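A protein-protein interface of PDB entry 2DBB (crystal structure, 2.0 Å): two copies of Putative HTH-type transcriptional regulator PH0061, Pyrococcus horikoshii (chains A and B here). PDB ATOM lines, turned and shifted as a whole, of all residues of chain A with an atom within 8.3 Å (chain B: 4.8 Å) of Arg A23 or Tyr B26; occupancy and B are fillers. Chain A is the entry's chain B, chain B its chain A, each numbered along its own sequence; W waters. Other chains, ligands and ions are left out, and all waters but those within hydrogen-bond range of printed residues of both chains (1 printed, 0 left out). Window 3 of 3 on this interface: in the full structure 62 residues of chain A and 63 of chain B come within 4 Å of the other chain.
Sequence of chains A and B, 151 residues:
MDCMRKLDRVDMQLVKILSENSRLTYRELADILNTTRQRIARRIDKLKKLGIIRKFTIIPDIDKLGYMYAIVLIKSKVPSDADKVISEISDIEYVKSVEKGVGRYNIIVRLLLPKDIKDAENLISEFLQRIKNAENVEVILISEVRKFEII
OG of Ser A22 lies within hydrogen-bond range of OG of Ser B22 (2.6 Å).
The backbone carbonyl oxygen (O) of Ser B22 sits at hydrogen-bond distance from the guanidinium group (NH1) of Arg A23, 2.5 Å away.
The backbone carbonyl oxygen (O) of Phe A56 sits at hydrogen-bond distance from the backbone NH (N) of Ser B22 (2.8 Å).
The backbone carbonyl oxygen of Thr A57 sits at hydrogen-bond distance from the side-chain hydroxyl of Ser B22 (3.3 Å).
O of Ser A22 is in hydrogen-bond range of NH1 of Arg B23 (2.7 Å).
O of Leu A24 is in hydrogen-bond range of NH1 of Arg B23 (2.9 Å).
O of Leu B24 is in hydrogen-bond range of NH1 of Arg A23, at 2.8 Å.
O of Phe B56 sits close to N of Asn A21, at 3.3 Å.
The backbone carbonyl oxygen (O) of Phe B56 lies within hydrogen-bond range of the backbone NH (N) of Ser A22.
O of Glu A20 lies close to O of Phe B56, 3.3 Å away.
The backbone NH (N) of Arg A23 sits close to the side-chain amide oxygen (OD1) of Asn A21.
Ser A19 touches Phe B56.
Arg A23 touches Arg B23 (NH1 to C, 3.6 Å).
CE1 of Tyr A26 touches NH2 of Arg B23, 3.7 Å away.
O of Phe A56 touches O of Leu B18 (3.8 Å).
CD of Arg B23 touches CE1 of Phe A56 (3.3 Å).
Leu B18 touches Thr A57 (O to CA, 3.7 Å).
C of Phe B56 touches O of Thr A57 (3.8 Å).
O of Leu B18 touches CG2 of Ile A58, 3.8 Å away.
Ile A58 touches Ser B22 (CG2 to CB, 3.9 Å).
Phe B56 touches Ile A58 (CD1 to CG2, 3.6 Å).
Arg A23 touches just these residues of chain B: Ser B22, Arg B23, Leu B24, Tyr B26 and Phe B56.
Tyr B26 touches one residue of chain A.
Of the printed residues of chain A, Leu B18 touches Phe A56, Thr A57 and Ile A58.
Of the printed residues of chain A, Ser B22 touches Ser A22 (2.6 Å), Arg A23 (2.5 Å), Phe A56 (2.8 Å), Thr A57 (3.3 Å) and Ile A58 (3.9 Å).
The nearest printed residue of chain A that does not touch Tyr B26 is Asn A21 (9.7 Å).
The nearest printed residue of chain A that does not touch Phe B56 is Ile A17 (5.8 Å).
Printed residues of chain B that touch a printed residue of chain A: Leu B18, Ser B22, Arg B23, Leu B24, Tyr B26 and Phe B56.
Hydrophobic or aromatic side chains of chain B within 4 Å of the printed part of chain A: Leu B18, Tyr B26 and Phe B56.
Among the printed residues, 23 pairs touch across the chains.
Among the printed residues, no Asp or Glu carboxylate lies within 4 Å of a Lys or Arg side-chain nitrogen of the other chain.
Leu A18 touches Phe B56, and with the chains exchanged Phe A56 touches Leu B18.
Ser A22 touches its own counterpart, Ser B22.
Ser A22 touches Phe B56, and with the chains exchanged Phe A56 touches Ser B22.
Arg B23 touches its own counterpart, Arg A23.
Water W1 lies within hydrogen-bond range of O of Glu A20 (2.6 Å) and N of Phe B56 (2.9 Å).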
ATOM      1  N   ILE A  17     -13.087  -6.371  16.966  1.00  0.00           N
ATOM      2  CA  ILE A  17     -13.295  -7.812  16.880  1.00  0.00           C
ATOM      3  C   ILE A  17     -11.988  -8.605  16.869  1.00  0.00           C
ATOM      4  O   ILE A  17     -11.834  -9.562  17.628  1.00  0.00           O
ATOM      5  CB  ILE A  17     -14.131  -8.163  15.629  1.00  0.00           C
ATOM      6  CG1 ILE A  17     -15.509  -7.496  15.739  1.00  0.00           C
ATOM      7  CG2 ILE A  17     -14.286  -9.680  15.497  1.00  0.00           C
ATOM      8  CD1 ILE A  17     -16.389  -7.668  14.518  1.00  0.00           C
ATOM      9  N   LEU A  18     -11.052  -8.201  16.018  1.00  0.00           N
ATOM     10  CA  LEU A  18      -9.761  -8.871  15.908  1.00  0.00           C
ATOM     11  C   LEU A  18      -8.962  -8.840  17.199  1.00  0.00           C
ATOM     12  O   LEU A  18      -8.104  -9.695  17.424  1.00  0.00           O
ATOM     13  CB  LEU A  18      -8.932  -8.234  14.792  1.00  0.00           C
ATOM     14  CG  LEU A  18      -9.463  -8.492  13.381  1.00  0.00           C
ATOM     15  CD1 LEU A  18      -8.640  -7.724  12.368  1.00  0.00           C
ATOM     16  CD2 LEU A  18      -9.421  -9.986  13.102  1.00  0.00           C
ATOM     17  N   SER A  19      -9.237  -7.854  18.044  1.00  0.00           N
ATOM     18  CA  SER A  19      -8.530  -7.747  19.305  1.00  0.00           C
ATOM     19  C   SER A  19      -9.006  -8.806  20.300  1.00  0.00           C
ATOM     20  O   SER A  19      -8.289  -9.124  21.251  1.00  0.00           O
ATOM     21  CB  SER A  19      -8.689  -6.335  19.896  1.00  0.00           C
ATOM     22  OG  SER A  19     -10.033  -6.051  20.244  1.00  0.00           O
ATOM     23  N   GLU A  20     -10.200  -9.360  20.072  1.00  0.00           N
ATOM     24  CA  GLU A  20     -10.753 -10.401  20.947  1.00  0.00           C
ATOM     25  C   GLU A  20     -10.471 -11.793  20.376  1.00  0.00           C
ATOM     26  O   GLU A  20     -10.313 -12.761  21.129  1.00  0.00           O
ATOM     27  CB  GLU A  20     -12.269 -10.232  21.122  1.00  0.00           C
ATOM     28  CG  GLU A  20     -12.700  -9.040  21.973  1.00  0.00           C
ATOM     29  CD  GLU A  20     -12.179  -9.097  23.409  1.00  0.00           C
ATOM     30  OE1 GLU A  20     -11.985 -10.208  23.955  1.00  0.00           O
ATOM     31  OE2 GLU A  20     -11.981  -8.017  24.005  1.00  0.00           O
ATOM     32  N   ASN A  21     -10.422 -11.889  19.047  1.00  0.00           N
ATOM     33  CA  ASN A  21     -10.136 -13.152  18.368  1.00  0.00           C
ATOM     34  C   ASN A  21      -9.465 -12.876  17.023  1.00  0.00           C
ATOM     35  O   ASN A  21     -10.127 -12.786  15.989  1.00  0.00           O
ATOM     36  CB  ASN A  21     -11.418 -13.961  18.141  1.00  0.00           C
ATOM     37  CG  ASN A  21     -11.135 -15.378  17.677  1.00  0.00           C
ATOM     38  OD1 ASN A  21     -10.022 -15.692  17.250  1.00  0.00           O
ATOM     39  ND2 ASN A  21     -12.146 -16.239  17.748  1.00  0.00           N
ATOM     40  N   SER A  22      -8.142 -12.767  17.047  1.00  0.00           N
ATOM     41  CA  SER A  22      -7.378 -12.476  15.851  1.00  0.00           C
ATOM     42  C   SER A  22      -7.313 -13.612  14.836  1.00  0.00           C
ATOM     43  O   SER A  22      -6.712 -13.445  13.775  1.00  0.00           O
ATOM     44  CB  SER A  22      -5.956 -12.068  16.240  1.00  0.00           C
ATOM     45  OG  SER A  22      -5.271 -13.156  16.839  1.00  0.00           O
ATOM     46  N   ARG A  23      -7.911 -14.762  15.145  1.00  0.00           N
ATOM     47  CA  ARG A  23      -7.873 -15.888  14.209  1.00  0.00           C
ATOM     48  C   ARG A  23      -9.156 -16.083  13.410  1.00  0.00           C
ATOM     49  O   ARG A  23      -9.285 -17.053  12.670  1.00  0.00           O
ATOM     50  CB  ARG A  23      -7.518 -17.197  14.933  1.00  0.00           C
ATOM     51  CG  ARG A  23      -6.085 -17.262  15.435  1.00  0.00           C
ATOM     52  CD  ARG A  23      -5.741 -18.653  15.978  1.00  0.00           C
ATOM     53  NE  ARG A  23      -5.732 -19.670  14.926  1.00  0.00           N
ATOM     54  CZ  ARG A  23      -4.698 -19.928  14.129  1.00  0.00           C
ATOM     55  NH1 ARG A  23      -3.563 -19.249  14.253  1.00  0.00           N
ATOM     56  NH2 ARG A  23      -4.801 -20.865  13.195  1.00  0.00           N
ATOM     57  N   LEU A  24     -10.105 -15.167  13.550  1.00  0.00           N
ATOM     58  CA  LEU A  24     -11.350 -15.271  12.801  1.00  0.00           C
ATOM     59  C   LEU A  24     -11.057 -15.165  11.302  1.00  0.00           C
ATOM     60  O   LEU A  24     -10.359 -14.257  10.865  1.00  0.00           O
ATOM     61  CB  LEU A  24     -12.313 -14.160  13.230  1.00  0.00           C
ATOM     62  CG  LEU A  24     -12.905 -14.335  14.630  1.00  0.00           C
ATOM     63  CD1 LEU A  24     -13.538 -13.036  15.095  1.00  0.00           C
ATOM     64  CD2 LEU A  24     -13.923 -15.464  14.609  1.00  0.00           C
ATOM     65  N   THR A  25     -11.581 -16.105  10.520  1.00  0.00           N
ATOM     66  CA  THR A  25     -11.374 -16.103   9.072  1.00  0.00           C
ATOM     67  C   THR A  25     -12.151 -14.943   8.457  1.00  0.00           C
ATOM     68  O   THR A  25     -13.100 -14.443   9.069  1.00  0.00           O
ATOM     69  CB  THR A  25     -11.880 -17.412   8.426  1.00  0.00           C
ATOM     70  OG1 THR A  25     -13.307 -17.491   8.563  1.00  0.00           O
ATOM     71  CG2 THR A  25     -11.249 -18.622   9.103  1.00  0.00           C
ATOM     72  N   TYR A  26     -11.755 -14.520   7.254  1.00  0.00           N
ATOM     73  CA  TYR A  26     -12.439 -13.418   6.577  1.00  0.00           C
ATOM     74  C   TYR A  26     -13.927 -13.734   6.406  1.00  0.00           C
ATOM     75  O   TYR A  26     -14.778 -12.845   6.447  1.00  0.00           O
ATOM     76  CB  TYR A  26     -11.814 -13.150   5.201  1.00  0.00           C
ATOM     77  CG  TYR A  26     -10.367 -12.704   5.248  1.00  0.00           C
ATOM     78  CD1 TYR A  26      -9.841 -12.108   6.392  1.00  0.00           C
ATOM     79  CD2 TYR A  26      -9.530 -12.860   4.144  1.00  0.00           C
ATOM     80  CE1 TYR A  26      -8.523 -11.678   6.443  1.00  0.00           C
ATOM     81  CE2 TYR A  26      -8.195 -12.425   4.183  1.00  0.00           C
ATOM     82  CZ  TYR A  26      -7.704 -11.836   5.341  1.00  0.00           C
ATOM     83  OH  TYR A  26      -6.400 -11.406   5.415  1.00  0.00           O
ATOM     84  N   GLU A  28     -15.868 -15.621   8.470  1.00  0.00           N
ATOM     85  CA  GLU A  28     -16.542 -15.395   9.748  1.00  0.00           C
ATOM     86  C   GLU A  28     -16.712 -13.890   9.988  1.00  0.00           C
ATOM     87  O   GLU A  28     -17.763 -13.434  10.441  1.00  0.00           O
ATOM     88  CB  GLU A  28     -15.731 -15.999  10.902  1.00  0.00           C
ATOM     89  CG  GLU A  28     -15.739 -17.520  10.981  1.00  0.00           C
ATOM     90  CD  GLU A  28     -14.817 -18.041  12.075  1.00  0.00           C
ATOM     91  OE1 GLU A  28     -13.579 -17.906  11.931  1.00  0.00           O
ATOM     92  OE2 GLU A  28     -15.326 -18.572  13.087  1.00  0.00           O
ATOM     93  N   LEU A  29     -15.671 -13.118   9.693  1.00  0.00           N
ATOM     94  CA  LEU A  29     -15.739 -11.669   9.873  1.00  0.00           C
ATOM     95  C   LEU A  29     -16.824 -11.082   8.971  1.00  0.00           C
ATOM     96  O   LEU A  29     -17.619 -10.245   9.404  1.00  0.00           O
ATOM     97  CB  LEU A  29     -14.387 -11.026   9.544  1.00  0.00           C
ATOM     98  CG  LEU A  29     -13.238 -11.371  10.494  1.00  0.00           C
ATOM     99  CD1 LEU A  29     -11.925 -10.891   9.910  1.00  0.00           C
ATOM    100  CD2 LEU A  29     -13.497 -10.729  11.851  1.00  0.00           C
ATOM    101  N   PHE A  56      -0.266  -9.455  14.859  1.00  0.00           N
ATOM    102  CA  PHE A  56      -1.274 -10.444  15.228  1.00  0.00           C
ATOM    103  C   PHE A  56      -0.540 -11.271  16.269  1.00  0.00           C
ATOM    104  O   PHE A  56       0.365 -12.035  15.932  1.00  0.00           O
ATOM    105  CB  PHE A  56      -1.650 -11.318  14.026  1.00  0.00           C
ATOM    106  CG  PHE A  56      -2.495 -10.614  13.010  1.00  0.00           C
ATOM    107  CD1 PHE A  56      -3.879 -10.585  13.138  1.00  0.00           C
ATOM    108  CD2 PHE A  56      -1.909  -9.945  11.944  1.00  0.00           C
ATOM    109  CE1 PHE A  56      -4.671  -9.895  12.216  1.00  0.00           C
ATOM    110  CE2 PHE A  56      -2.689  -9.251  11.016  1.00  0.00           C
ATOM    111  CZ  PHE A  56      -4.075  -9.228  11.155  1.00  0.00           C
ATOM    112  N   THR A  57      -0.914 -11.109  17.533  1.00  0.00           N
ATOM    113  CA  THR A  57      -0.232 -11.818  18.604  1.00  0.00           C
ATOM    114  C   THR A  57      -1.201 -12.475  19.592  1.00  0.00           C
ATOM    115  O   THR A  57      -2.386 -12.645  19.293  1.00  0.00           O
ATOM    116  CB  THR A  57       0.726 -10.842  19.346  1.00  0.00           C
ATOM    117  OG1 THR A  57       1.551 -11.564  20.269  1.00  0.00           O
ATOM    118  CG2 THR A  57      -0.067  -9.784  20.092  1.00  0.00           C
ATOM    119  N   ILE A  58      -0.692 -12.856  20.760  1.00  0.00           N
ATOM    120  CA  ILE A  58      -1.516 -13.498  21.778  1.00  0.00           C
ATOM    121  C   ILE A  58      -1.292 -12.898  23.155  1.00  0.00           C
ATOM    122  O   ILE A  58      -0.278 -12.244  23.402  1.00  0.00           O
ATOM    123  CB  ILE A  58      -1.198 -15.007  21.899  1.00  0.00           C
ATOM    124  CG1 ILE A  58       0.277 -15.197  22.276  1.00  0.00           C
ATOM    125  CG2 ILE A  58      -1.509 -15.718  20.592  1.00  0.00           C
ATOM    126  CD1 ILE A  58       0.655 -16.634  22.610  1.00  0.00           C
ATOM    127  N   LEU B  18       3.259 -18.094  17.878  1.00  0.00           N
ATOM    128  CA  LEU B  18       1.962 -17.434  17.887  1.00  0.00           C
ATOM    129  C   LEU B  18       2.062 -15.991  18.391  1.00  0.00           C
ATOM    130  O   LEU B  18       1.247 -15.142  18.027  1.00  0.00           O
ATOM    131  CB  LEU B  18       0.971 -18.241  18.737  1.00  0.00           C
ATOM    132  CG  LEU B  18       0.539 -19.595  18.147  1.00  0.00           C
ATOM    133  CD1 LEU B  18      -0.226 -20.397  19.183  1.00  0.00           C
ATOM    134  CD2 LEU B  18      -0.324 -19.371  16.921  1.00  0.00           C
ATOM    135  N   SER B  22      -0.143 -14.720  15.246  1.00  0.00           N
ATOM    136  CA  SER B  22      -1.207 -15.576  15.749  1.00  0.00           C
ATOM    137  C   SER B  22      -2.179 -16.084  14.687  1.00  0.00           C
ATOM    138  O   SER B  22      -3.059 -16.877  15.008  1.00  0.00           O
ATOM    139  CB  SER B  22      -1.994 -14.849  16.844  1.00  0.00           C
ATOM    140  OG  SER B  22      -2.811 -13.835  16.283  1.00  0.00           O
ATOM    141  N   ARG B  23      -2.038 -15.628  13.443  1.00  0.00           N
ATOM    142  CA  ARG B  23      -2.929 -16.079  12.375  1.00  0.00           C
ATOM    143  C   ARG B  23      -2.326 -17.191  11.524  1.00  0.00           C
ATOM    144  O   ARG B  23      -2.834 -17.490  10.443  1.00  0.00           O
ATOM    145  CB  ARG B  23      -3.333 -14.922  11.447  1.00  0.00           C
ATOM    146  CG  ARG B  23      -4.395 -13.989  12.007  1.00  0.00           C
ATOM    147  CD  ARG B  23      -4.832 -12.944  10.967  1.00  0.00           C
ATOM    148  NE  ARG B  23      -5.712 -13.483   9.929  1.00  0.00           N
ATOM    149  CZ  ARG B  23      -7.009 -13.734  10.099  1.00  0.00           C
ATOM    150  NH1 ARG B  23      -7.593 -13.501  11.270  1.00  0.00           N
ATOM    151  NH2 ARG B  23      -7.728 -14.207   9.092  1.00  0.00           N
ATOM    152  N   LEU B  24      -1.238 -17.795  11.994  1.00  0.00           N
ATOM    153  CA  LEU B  24      -0.612 -18.880  11.248  1.00  0.00           C
ATOM    154  C   LEU B  24      -1.547 -20.077  11.190  1.00  0.00           C
ATOM    155  O   LEU B  24      -2.175 -20.440  12.187  1.00  0.00           O
ATOM    156  CB  LEU B  24       0.712 -19.299  11.896  1.00  0.00           C
ATOM    157  CG  LEU B  24       1.907 -18.391  11.587  1.00  0.00           C
ATOM    158  CD1 LEU B  24       3.122 -18.835  12.371  1.00  0.00           C
ATOM    159  CD2 LEU B  24       2.195 -18.433  10.096  1.00  0.00           C
ATOM    160  N   THR B  25      -1.647 -20.682  10.013  1.00  0.00           N
ATOM    161  CA  THR B  25      -2.496 -21.851   9.832  1.00  0.00           C
ATOM    162  C   THR B  25      -1.830 -23.033  10.527  1.00  0.00           C
ATOM    163  O   THR B  25      -0.604 -23.061  10.678  1.00  0.00           O
ATOM    164  CB  THR B  25      -2.665 -22.181   8.336  1.00  0.00           C
ATOM    165  OG1 THR B  25      -1.388 -22.512   7.771  1.00  0.00           O
ATOM    166  CG2 THR B  25      -3.241 -20.982   7.588  1.00  0.00           C
ATOM    167  N   TYR B  26      -2.632 -23.999  10.964  1.00  0.00           N
ATOM    168  CA  TYR B  26      -2.088 -25.179  11.628  1.00  0.00           C
ATOM    169  C   TYR B  26      -1.077 -25.855  10.705  1.00  0.00           C
ATOM    170  O   TYR B  26      -0.118 -26.474  11.160  1.00  0.00           O
ATOM    171  CB  TYR B  26      -3.206 -26.163  11.978  1.00  0.00           C
ATOM    172  CG  TYR B  26      -4.069 -25.741  13.149  1.00  0.00           C
ATOM    173  CD1 TYR B  26      -3.682 -24.697  13.988  1.00  0.00           C
ATOM    174  CD2 TYR B  26      -5.258 -26.410  13.438  1.00  0.00           C
ATOM    175  CE1 TYR B  26      -4.453 -24.329  15.086  1.00  0.00           C
ATOM    176  CE2 TYR B  26      -6.039 -26.051  14.536  1.00  0.00           C
ATOM    177  CZ  TYR B  26      -5.627 -25.008  15.355  1.00  0.00           C
ATOM    178  OH  TYR B  26      -6.387 -24.647  16.442  1.00  0.00           O
ATOM    179  N   ARG B  27      -1.310 -25.728   9.402  1.00  0.00           N
ATOM    180  CA  ARG B  27      -0.428 -26.304   8.399  1.00  0.00           C
ATOM    181  C   ARG B  27       0.940 -25.647   8.519  1.00  0.00           C
ATOM    182  O   ARG B  27       1.963 -26.323   8.594  1.00  0.00           O
ATOM    183  CB  ARG B  27      -1.002 -26.063   6.996  1.00  0.00           C
ATOM    184  CG  ARG B  27       0.050 -25.785   5.932  1.00  0.00           C
ATOM    185  CD  ARG B  27      -0.580 -25.333   4.629  1.00  0.00           C
ATOM    186  NE  ARG B  27      -1.150 -26.448   3.879  1.00  0.00           N
ATOM    187  CZ  ARG B  27      -0.696 -26.856   2.698  1.00  0.00           C
ATOM    188  NH1 ARG B  27      -1.271 -27.883   2.082  1.00  0.00           N
ATOM    189  NH2 ARG B  27       0.327 -26.230   2.129  1.00  0.00           N
ATOM    190  N   GLU B  28       0.945 -24.319   8.534  1.00  0.00           N
ATOM    191  CA  GLU B  28       2.188 -23.571   8.646  1.00  0.00           C
ATOM    192  C   GLU B  28       2.889 -23.862   9.967  1.00  0.00           C
ATOM    193  O   GLU B  28       4.119 -23.932  10.020  1.00  0.00           O
ATOM    194  CB  GLU B  28       1.908 -22.073   8.519  1.00  0.00           C
ATOM    195  CG  GLU B  28       1.482 -21.646   7.124  1.00  0.00           C
ATOM    196  CD  GLU B  28       1.179 -20.160   7.035  1.00  0.00           C
ATOM    197  OE1 GLU B  28       0.154 -19.724   7.604  1.00  0.00           O
ATOM    198  OE2 GLU B  28       1.976 -19.427   6.404  1.00  0.00           O
ATOM    199  N   LEU B  29       2.105 -24.040  11.028  1.00  0.00           N
ATOM    200  CA  LEU B  29       2.658 -24.326  12.346  1.00  0.00           C
ATOM    201  C   LEU B  29       3.280 -25.720  12.391  1.00  0.00           C
ATOM    202  O   LEU B  29       4.369 -25.907  12.929  1.00  0.00           O
ATOM    203  CB  LEU B  29       1.571 -24.203  13.422  1.00  0.00           C
ATOM    204  CG  LEU B  29       0.978 -22.809  13.670  1.00  0.00           C
ATOM    205  CD1 LEU B  29      -0.147 -22.908  14.689  1.00  0.00           C
ATOM    206  CD2 LEU B  29       2.067 -21.859  14.163  1.00  0.00           C
ATOM    207  N   ALA B  30       2.584 -26.697  11.821  1.00  0.00           N
ATOM    208  CA  ALA B  30       3.089 -28.063  11.794  1.00  0.00           C
ATOM    209  C   ALA B  30       4.415 -28.092  11.032  1.00  0.00           C
ATOM    210  O   ALA B  30       5.358 -28.753  11.449  1.00  0.00           O
ATOM    211  CB  ALA B  30       2.073 -28.988  11.128  1.00  0.00           C
ATOM    212  N   ARG B  37      -0.644 -31.386  11.625  1.00  0.00           N
ATOM    213  CA  ARG B  37      -1.685 -30.418  11.938  1.00  0.00           C
ATOM    214  C   ARG B  37      -2.567 -30.947  13.058  1.00  0.00           C
ATOM    215  O   ARG B  37      -3.083 -30.181  13.871  1.00  0.00           O
ATOM    216  CB  ARG B  37      -2.521 -30.116  10.691  1.00  0.00           C
ATOM    217  CG  ARG B  37      -1.785 -29.249   9.682  1.00  0.00           C
ATOM    218  CD  ARG B  37      -2.602 -28.958   8.431  1.00  0.00           C
ATOM    219  NE  ARG B  37      -2.766 -30.140   7.591  1.00  0.00           N
ATOM    220  CZ  ARG B  37      -3.142 -30.104   6.316  1.00  0.00           C
ATOM    221  NH1 ARG B  37      -3.390 -28.941   5.726  1.00  0.00           N
ATOM    222  NH2 ARG B  37      -3.272 -31.233   5.629  1.00  0.00           N
ATOM    223  N   ILE B  40      -0.763 -30.167  16.242  1.00  0.00           N
ATOM    224  CA  ILE B  40      -0.785 -28.732  16.480  1.00  0.00           C
ATOM    225  C   ILE B  40      -2.145 -28.356  17.062  1.00  0.00           C
ATOM    226  O   ILE B  40      -2.232 -27.663  18.075  1.00  0.00           O
ATOM    227  CB  ILE B  40      -0.550 -27.959  15.167  1.00  0.00           C
ATOM    228  CG1 ILE B  40       0.891 -28.173  14.696  1.00  0.00           C
ATOM    229  CG2 ILE B  40      -0.833 -26.482  15.362  1.00  0.00           C
ATOM    230  CD1 ILE B  40       1.938 -27.663  15.663  1.00  0.00           C
ATOM    231  N   ALA B  41      -3.207 -28.832  16.421  1.00  0.00           N
ATOM    232  CA  ALA B  41      -4.564 -28.556  16.878  1.00  0.00           C
ATOM    233  C   ALA B  41      -4.737 -28.982  18.335  1.00  0.00           C
ATOM    234  O   ALA B  41      -5.336 -28.264  19.132  1.00  0.00           O
ATOM    235  CB  ALA B  41      -5.574 -29.288  15.988  1.00  0.00           C
ATOM    236  N   ILE B  44      -2.492 -26.610  20.836  1.00  0.00           N
ATOM    237  CA  ILE B  44      -3.123 -25.313  21.006  1.00  0.00           C
ATOM    238  C   ILE B  44      -4.404 -25.449  21.824  1.00  0.00           C
ATOM    239  O   ILE B  44      -4.715 -24.589  22.649  1.00  0.00           O
ATOM    240  CB  ILE B  44      -3.447 -24.665  19.649  1.00  0.00           C
ATOM    241  CG1 ILE B  44      -2.145 -24.330  18.923  1.00  0.00           C
ATOM    242  CG2 ILE B  44      -4.286 -23.404  19.854  1.00  0.00           C
ATOM    243  CD1 ILE B  44      -2.348 -23.651  17.590  1.00  0.00           C
ATOM    244  N   PHE B  56      -6.311 -14.532  21.500  1.00  0.00           N
ATOM    245  CA  PHE B  56      -5.677 -14.303  20.211  1.00  0.00           C
ATOM    246  C   PHE B  56      -6.119 -12.879  19.920  1.00  0.00           C
ATOM    247  O   PHE B  56      -7.306 -12.623  19.713  1.00  0.00           O
ATOM    248  CB  PHE B  56      -6.224 -15.275  19.167  1.00  0.00           C
ATOM    249  CG  PHE B  56      -5.744 -16.687  19.357  1.00  0.00           C
ATOM    250  CD1 PHE B  56      -4.460 -17.054  18.963  1.00  0.00           C
ATOM    251  CD2 PHE B  56      -6.552 -17.633  19.982  1.00  0.00           C
ATOM    252  CE1 PHE B  56      -3.984 -18.349  19.190  1.00  0.00           C
ATOM    253  CE2 PHE B  56      -6.087 -18.929  20.217  1.00  0.00           C
ATOM    254  CZ  PHE B  56      -4.802 -19.289  19.822  1.00  0.00           C
HETATM  255  O   HOH W   1      -9.114 -15.039  21.283  1.00  0.00           O
